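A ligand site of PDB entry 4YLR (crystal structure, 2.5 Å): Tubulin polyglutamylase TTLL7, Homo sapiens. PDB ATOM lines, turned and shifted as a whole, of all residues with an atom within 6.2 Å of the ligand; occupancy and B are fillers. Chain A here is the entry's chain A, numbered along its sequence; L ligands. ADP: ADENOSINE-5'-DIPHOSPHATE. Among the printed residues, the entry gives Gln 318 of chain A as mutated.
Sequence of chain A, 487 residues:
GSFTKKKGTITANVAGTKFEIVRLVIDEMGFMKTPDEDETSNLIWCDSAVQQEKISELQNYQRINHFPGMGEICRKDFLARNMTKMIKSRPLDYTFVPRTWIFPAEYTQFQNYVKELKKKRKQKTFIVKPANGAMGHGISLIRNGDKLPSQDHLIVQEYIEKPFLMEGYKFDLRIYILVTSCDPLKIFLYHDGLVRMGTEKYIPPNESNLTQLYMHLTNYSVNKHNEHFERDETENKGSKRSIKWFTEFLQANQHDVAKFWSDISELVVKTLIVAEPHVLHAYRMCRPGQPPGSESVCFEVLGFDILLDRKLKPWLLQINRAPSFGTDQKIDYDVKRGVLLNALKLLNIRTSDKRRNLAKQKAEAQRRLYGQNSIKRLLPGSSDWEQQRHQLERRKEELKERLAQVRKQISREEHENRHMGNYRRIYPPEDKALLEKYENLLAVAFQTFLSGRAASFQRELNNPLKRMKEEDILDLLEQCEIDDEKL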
ATOM      1  N   LYS A  76     -10.392  16.589  18.087  1.00  0.00           N
ATOM      2  CA  LYS A  76     -10.986  16.993  16.819  1.00  0.00           C
ATOM      3  C   LYS A  76     -10.764  15.972  15.706  1.00  0.00           C
ATOM      4  O   LYS A  76     -11.595  15.824  14.812  1.00  0.00           O
ATOM      5  CB  LYS A  76     -10.428  18.346  16.380  1.00  0.00           C
ATOM      6  CG  LYS A  76     -10.660  19.465  17.378  1.00  0.00           C
ATOM      7  CD  LYS A  76      -9.933  20.738  16.964  1.00  0.00           C
ATOM      8  CE  LYS A  76      -9.712  21.658  18.146  1.00  0.00           C
ATOM      9  NZ  LYS A  76      -8.844  22.817  17.795  1.00  0.00           N
ATOM     10  N   PRO A  98     -19.965  19.864   9.952  1.00  0.00           N
ATOM     11  CA  PRO A  98     -19.359  20.296   8.681  1.00  0.00           C
ATOM     12  C   PRO A  98     -18.344  19.268   8.193  1.00  0.00           C
ATOM     13  O   PRO A  98     -17.669  18.650   9.022  1.00  0.00           O
ATOM     14  CB  PRO A  98     -18.678  21.620   9.042  1.00  0.00           C
ATOM     15  CG  PRO A  98     -18.450  21.547  10.513  1.00  0.00           C
ATOM     16  CD  PRO A  98     -19.600  20.757  11.064  1.00  0.00           C
ATOM     17  N   ILE A 127     -11.539  25.947   6.329  1.00  0.00           N
ATOM     18  CA  ILE A 127     -10.768  26.380   7.487  1.00  0.00           C
ATOM     19  C   ILE A 127      -9.791  25.279   7.905  1.00  0.00           C
ATOM     20  O   ILE A 127     -10.097  24.094   7.811  1.00  0.00           O
ATOM     21  CB  ILE A 127     -11.685  26.767   8.669  1.00  0.00           C
ATOM     22  CG1 ILE A 127     -10.874  27.385   9.814  1.00  0.00           C
ATOM     23  CG2 ILE A 127     -12.504  25.570   9.148  1.00  0.00           C
ATOM     24  CD1 ILE A 127     -11.720  27.888  10.965  1.00  0.00           C
ATOM     25  N   LYS A 129      -7.512  23.788  10.990  1.00  0.00           N
ATOM     26  CA  LYS A 129      -7.354  23.805  12.441  1.00  0.00           C
ATOM     27  C   LYS A 129      -6.129  23.013  12.875  1.00  0.00           C
ATOM     28  O   LYS A 129      -5.731  22.057  12.216  1.00  0.00           O
ATOM     29  CB  LYS A 129      -8.610  23.262  13.125  1.00  0.00           C
ATOM     30  CG  LYS A 129      -9.877  24.032  12.789  1.00  0.00           C
ATOM     31  CD  LYS A 129     -11.104  23.410  13.452  1.00  0.00           C
ATOM     32  CE  LYS A 129     -12.366  24.171  13.102  1.00  0.00           C
ATOM     33  NZ  LYS A 129     -13.575  23.587  13.763  1.00  0.00           N
ATOM     34  N   PRO A 130      -5.532  23.419  14.007  1.00  0.00           N
ATOM     35  CA  PRO A 130      -4.340  22.803  14.590  1.00  0.00           C
ATOM     36  C   PRO A 130      -4.575  21.340  14.981  1.00  0.00           C
ATOM     37  O   PRO A 130      -5.691  20.995  15.357  1.00  0.00           O
ATOM     38  CB  PRO A 130      -4.063  23.657  15.836  1.00  0.00           C
ATOM     39  N   ILE A 139      -4.401  28.642  12.888  1.00  0.00           N
ATOM     40  CA  ILE A 139      -5.681  28.515  12.200  1.00  0.00           C
ATOM     41  C   ILE A 139      -5.802  29.506  11.057  1.00  0.00           C
ATOM     42  O   ILE A 139      -5.622  30.716  11.249  1.00  0.00           O
ATOM     43  CB  ILE A 139      -6.861  28.715  13.173  1.00  0.00           C
ATOM     44  CG1 ILE A 139      -6.743  27.774  14.376  1.00  0.00           C
ATOM     45  CG2 ILE A 139      -8.190  28.502  12.458  1.00  0.00           C
ATOM     46  CD1 ILE A 139      -6.083  28.399  15.587  1.00  0.00           C
ATOM     47  N   GLN A 157     -11.646  21.561   7.239  1.00  0.00           N
ATOM     48  CA  GLN A 157     -13.080  21.580   7.466  1.00  0.00           C
ATOM     49  C   GLN A 157     -13.751  22.613   6.567  1.00  0.00           C
ATOM     50  O   GLN A 157     -13.204  23.695   6.354  1.00  0.00           O
ATOM     51  CB  GLN A 157     -13.385  21.865   8.938  1.00  0.00           C
ATOM     52  CG  GLN A 157     -14.819  21.620   9.348  1.00  0.00           C
ATOM     53  CD  GLN A 157     -15.020  21.768  10.851  1.00  0.00           C
ATOM     54  OE1 GLN A 157     -14.822  22.847  11.404  1.00  0.00           O
ATOM     55  NE2 GLN A 157     -15.390  20.678  11.507  1.00  0.00           N
ATOM     56  N   GLU A 158     -14.934  22.282   6.051  1.00  0.00           N
ATOM     57  CA  GLU A 158     -15.685  23.231   5.239  1.00  0.00           C
ATOM     58  C   GLU A 158     -16.088  24.428   6.093  1.00  0.00           C
ATOM     59  O   GLU A 158     -16.466  24.277   7.258  1.00  0.00           O
ATOM     60  CB  GLU A 158     -16.915  22.580   4.598  1.00  0.00           C
ATOM     61  CG  GLU A 158     -17.993  22.162   5.585  1.00  0.00           C
ATOM     62  CD  GLU A 158     -19.250  21.671   4.904  1.00  0.00           C
ATOM     63  OE1 GLU A 158     -19.229  21.476   3.670  1.00  0.00           O
ATOM     64  OE2 GLU A 158     -20.272  21.473   5.598  1.00  0.00           O
ATOM     65  N   TYR A 159     -15.993  25.616   5.514  1.00  0.00           N
ATOM     66  CA  TYR A 159     -16.235  26.843   6.271  1.00  0.00           C
ATOM     67  C   TYR A 159     -17.679  27.305   6.129  1.00  0.00           C
ATOM     68  O   TYR A 159     -18.138  27.593   5.021  1.00  0.00           O
ATOM     69  CB  TYR A 159     -15.275  27.952   5.798  1.00  0.00           C
ATOM     70  CG  TYR A 159     -15.354  29.222   6.609  1.00  0.00           C
ATOM     71  CD1 TYR A 159     -14.655  29.342   7.810  1.00  0.00           C
ATOM     72  CD2 TYR A 159     -16.115  30.300   6.183  1.00  0.00           C
ATOM     73  CE1 TYR A 159     -14.721  30.517   8.556  1.00  0.00           C
ATOM     74  CE2 TYR A 159     -16.183  31.466   6.926  1.00  0.00           C
ATOM     75  CZ  TYR A 159     -15.483  31.569   8.110  1.00  0.00           C
ATOM     76  OH  TYR A 159     -15.555  32.726   8.852  1.00  0.00           O
ATOM     77  N   ILE A 160     -18.408  27.349   7.247  1.00  0.00           N
ATOM     78  CA  ILE A 160     -19.743  27.924   7.247  1.00  0.00           C
ATOM     79  C   ILE A 160     -19.630  29.400   6.865  1.00  0.00           C
ATOM     80  O   ILE A 160     -19.215  30.238   7.670  1.00  0.00           O
ATOM     81  CB  ILE A 160     -20.445  27.775   8.619  1.00  0.00           C
ATOM     82  CG1 ILE A 160     -20.765  26.301   8.906  1.00  0.00           C
ATOM     83  CG2 ILE A 160     -21.734  28.583   8.663  1.00  0.00           C
ATOM     84  CD1 ILE A 160     -19.580  25.463   9.311  1.00  0.00           C
ATOM     85  N   GLU A 161     -19.982  29.711   5.624  1.00  0.00           N
ATOM     86  CA  GLU A 161     -19.753  31.036   5.062  1.00  0.00           C
ATOM     87  C   GLU A 161     -20.814  32.057   5.471  1.00  0.00           C
ATOM     88  O   GLU A 161     -20.526  33.246   5.570  1.00  0.00           O
ATOM     89  CB  GLU A 161     -19.668  30.961   3.542  1.00  0.00           C
ATOM     90  CG  GLU A 161     -18.351  30.399   3.014  1.00  0.00           C
ATOM     91  CD  GLU A 161     -18.382  30.102   1.533  1.00  0.00           C
ATOM     92  OE1 GLU A 161     -17.426  29.486   1.019  1.00  0.00           O
ATOM     93  OE2 GLU A 161     -19.375  30.484   0.865  1.00  0.00           O
ATOM     94  N   LYS A 170     -20.260  38.097  13.804  1.00  0.00           N
ATOM     95  CA  LYS A 170     -20.177  36.655  13.986  1.00  0.00           C
ATOM     96  C   LYS A 170     -19.890  36.338  15.452  1.00  0.00           C
ATOM     97  O   LYS A 170     -19.134  37.047  16.103  1.00  0.00           O
ATOM     98  CB  LYS A 170     -19.087  36.077  13.082  1.00  0.00           C
ATOM     99  CG  LYS A 170     -18.870  34.571  13.226  1.00  0.00           C
ATOM    100  CD  LYS A 170     -17.780  34.091  12.279  1.00  0.00           C
ATOM    101  CE  LYS A 170     -17.619  32.582  12.337  1.00  0.00           C
ATOM    102  NZ  LYS A 170     -16.598  32.105  11.373  1.00  0.00           N
ATOM    103  N   PHE A 171     -20.508  35.275  15.965  1.00  0.00           N
ATOM    104  CA  PHE A 171     -20.326  34.912  17.363  1.00  0.00           C
ATOM    105  C   PHE A 171     -20.243  33.400  17.565  1.00  0.00           C
ATOM    106  O   PHE A 171     -20.640  32.627  16.691  1.00  0.00           O
ATOM    107  CB  PHE A 171     -21.459  35.492  18.223  1.00  0.00           C
ATOM    108  CG  PHE A 171     -22.833  34.974  17.869  1.00  0.00           C
ATOM    109  CD1 PHE A 171     -23.375  33.899  18.545  1.00  0.00           C
ATOM    110  CD2 PHE A 171     -23.575  35.573  16.855  1.00  0.00           C
ATOM    111  CE1 PHE A 171     -24.634  33.423  18.223  1.00  0.00           C
ATOM    112  CE2 PHE A 171     -24.833  35.097  16.533  1.00  0.00           C
ATOM    113  CZ  PHE A 171     -25.363  34.029  17.209  1.00  0.00           C
ATOM    114  N   ASP A 172     -19.724  32.995  18.719  1.00  0.00           N
ATOM    115  CA  ASP A 172     -19.594  31.575  19.049  1.00  0.00           C
ATOM    116  C   ASP A 172     -20.475  31.206  20.236  1.00  0.00           C
ATOM    117  O   ASP A 172     -20.653  32.003  21.162  1.00  0.00           O
ATOM    118  CB  ASP A 172     -18.142  31.220  19.352  1.00  0.00           C
ATOM    119  CG  ASP A 172     -17.351  30.866  18.110  1.00  0.00           C
ATOM    120  OD1 ASP A 172     -17.073  29.666  17.912  1.00  0.00           O
ATOM    121  OD2 ASP A 172     -17.015  31.783  17.330  1.00  0.00           O
ATOM    122  N   ASP A 305     -18.540  23.751  21.737  1.00  0.00           N
ATOM    123  CA  ASP A 305     -18.395  24.943  20.913  1.00  0.00           C
ATOM    124  C   ASP A 305     -19.244  24.799  19.650  1.00  0.00           C
ATOM    125  O   ASP A 305     -19.034  23.882  18.861  1.00  0.00           O
ATOM    126  CB  ASP A 305     -16.927  25.187  20.550  1.00  0.00           C
ATOM    127  CG  ASP A 305     -16.071  25.501  21.770  1.00  0.00           C
ATOM    128  OD1 ASP A 305     -16.643  25.895  22.808  1.00  0.00           O
ATOM    129  OD2 ASP A 305     -14.835  25.380  21.679  1.00  0.00           O
ATOM    130  N   LEU A 307     -21.492  26.754  16.323  1.00  0.00           N
ATOM    131  CA  LEU A 307     -21.748  27.905  15.472  1.00  0.00           C
ATOM    132  C   LEU A 307     -23.087  27.764  14.740  1.00  0.00           C
ATOM    133  O   LEU A 307     -23.365  26.737  14.123  1.00  0.00           O
ATOM    134  CB  LEU A 307     -20.622  28.079  14.450  1.00  0.00           C
ATOM    135  CG  LEU A 307     -20.804  29.209  13.428  1.00  0.00           C
ATOM    136  CD1 LEU A 307     -20.812  30.565  14.113  1.00  0.00           C
ATOM    137  CD2 LEU A 307     -19.715  29.136  12.365  1.00  0.00           C
ATOM    138  N   LEU A 317     -18.535  22.318  16.391  1.00  0.00           N
ATOM    139  CA  LEU A 317     -17.151  22.638  16.080  1.00  0.00           C
ATOM    140  C   LEU A 317     -16.197  21.748  16.881  1.00  0.00           C
ATOM    141  O   LEU A 317     -15.338  21.071  16.303  1.00  0.00           O
ATOM    142  CB  LEU A 317     -16.851  24.111  16.364  1.00  0.00           C
ATOM    143  CG  LEU A 317     -17.585  25.126  15.483  1.00  0.00           C
ATOM    144  CD1 LEU A 317     -17.003  26.518  15.662  1.00  0.00           C
ATOM    145  CD2 LEU A 317     -17.537  24.693  14.016  1.00  0.00           C
ATOM    146  N   GLN A 318     -16.357  21.748  18.199  1.00  0.00           N
ATOM    147  CA  GLN A 318     -15.522  20.910  19.063  1.00  0.00           C
ATOM    148  C   GLN A 318     -16.189  20.642  20.398  1.00  0.00           C
ATOM    149  O   GLN A 318     -17.132  21.330  20.783  1.00  0.00           O
ATOM    150  CB  GLN A 318     -14.160  21.572  19.294  1.00  0.00           C
ATOM    151  CG  GLN A 318     -14.135  22.533  20.466  1.00  0.00           C
ATOM    152  CD  GLN A 318     -12.796  23.218  20.636  1.00  0.00           C
ATOM    153  OE1 GLN A 318     -11.960  23.195  19.727  1.00  0.00           O
ATOM    154  NE2 GLN A 318     -12.580  23.836  21.786  1.00  0.00           N
HETATM  155  PB  ADP L   1     -10.297  28.089  19.827  1.00  0.00           P
HETATM  156  O1B ADP L   1      -9.706  27.417  21.009  1.00  0.00           O
HETATM  157  O2B ADP L   1     -11.445  28.893  20.259  1.00  0.00           O
HETATM  158  O3B ADP L   1      -9.298  28.955  19.204  1.00  0.00           O
HETATM  159  PA  ADP L   1     -10.500  27.117  17.242  1.00  0.00           P
HETATM  160  O1A ADP L   1      -8.967  27.122  16.970  1.00  0.00           O
HETATM  161  O2A ADP L   1     -11.152  25.927  16.533  1.00  0.00           O
HETATM  162  O3A ADP L   1     -10.786  27.018  18.801  1.00  0.00           O
HETATM  163  O5' ADP L   1     -11.161  28.527  16.666  1.00  0.00           O
HETATM  164  C5' ADP L   1     -12.579  28.618  16.550  1.00  0.00           C
HETATM  165  C4' ADP L   1     -12.931  29.754  15.789  1.00  0.00           C
HETATM  166  O4' ADP L   1     -13.011  29.386  14.306  1.00  0.00           O
HETATM  167  C3' ADP L   1     -14.386  30.239  16.193  1.00  0.00           C
HETATM  168  O3' ADP L   1     -14.454  31.744  16.167  1.00  0.00           O
HETATM  169  C2' ADP L   1     -15.136  29.753  15.302  1.00  0.00           C
HETATM  170  O2' ADP L   1     -16.291  30.602  15.108  1.00  0.00           O
HETATM  171  C1' ADP L   1     -14.231  29.718  13.937  1.00  0.00           C
HETATM  172  N9  ADP L   1     -14.797  28.839  12.967  1.00  0.00           N
HETATM  173  C8  ADP L   1     -14.119  27.735  13.424  1.00  0.00           C
HETATM  174  N7  ADP L   1     -14.481  26.692  12.638  1.00  0.00           N
HETATM  175  C5  ADP L   1     -15.386  27.138  11.705  1.00  0.00           C
HETATM  176  C6  ADP L   1     -16.076  26.486  10.674  1.00  0.00           C
HETATM  177  N6  ADP L   1     -16.079  25.128  10.215  1.00  0.00           N
HETATM  178  N1  ADP L   1     -16.925  27.179   9.884  1.00  0.00           N
HETATM  179  C2  ADP L   1     -17.116  28.539  10.105  1.00  0.00           C
HETATM  180  N3  ADP L   1     -16.447  29.172  11.113  1.00  0.00           N
HETATM  181  C4  ADP L   1     -15.577  28.468  11.916  1.00  0.00           C
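OE1 of Gln 157 sits at hydrogen-bond distance from NZ of Lys 129 (2.8 Å). The backbone carbonyl oxygen (O) of Asp 305 is in hydrogen-bond range of the backbone NH (N) of Leu 317 (3.0 Å). N of Ile 127 lies within hydrogen-bond range of O of Gln 157 (2.8 Å). NZ of Lys 170 sits at hydrogen-bond distance from OH of Tyr 159, at 2.8 Å.
CD1 of Ile 127 touches C8 of the ligand, at 3.4 Å. Ile 139 touches the ligand (CD1 to O1A, 3.4 Å). Tyr 159 touches the ligand (CE1 to N3, 3.4 Å). CD2 of Leu 307 touches C2 of the ligand, at 3.5 Å. Leu 317 touches the ligand (CD1 to C2', 3.8 Å). Hydrophobic or aromatic side chains that line the ligand: Ile 127, Ile 139, Tyr 159, Ile 160, Leu 307 and Leu 317. 11 residues have an atom within 4 Å of the ligand: Ile 127, Lys 129, Ile 139, Gln 157, Glu 158, Tyr 159, Ile 160, Lys 170, Asp 172, Leu 307 and Leu 317.
The side-chain carboxylate (OD2) of Asp 172 is in hydrogen-bond range of an oxygen (O2') of the ligand, 2.6 Å away. NZ of Lys 129 lies close to N7 of the ligand (3.4 Å). A nitrogen (N6) of the ligand is in hydrogen-bond range of the backbone carbonyl oxygen (O) of Glu 158, at 3.1 Å. A nitrogen (N3) of the ligand lies within hydrogen-bond range of the side-chain amino group (NZ) of Lys 170 (2.9 Å). A nitrogen (N6) of the ligand is in hydrogen-bond range of the side-chain amide oxygen of Gln 157 (2.9 Å). A nitrogen (N1) of the ligand is in hydrogen-bond range of the backbone NH (N) of Ile 160.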
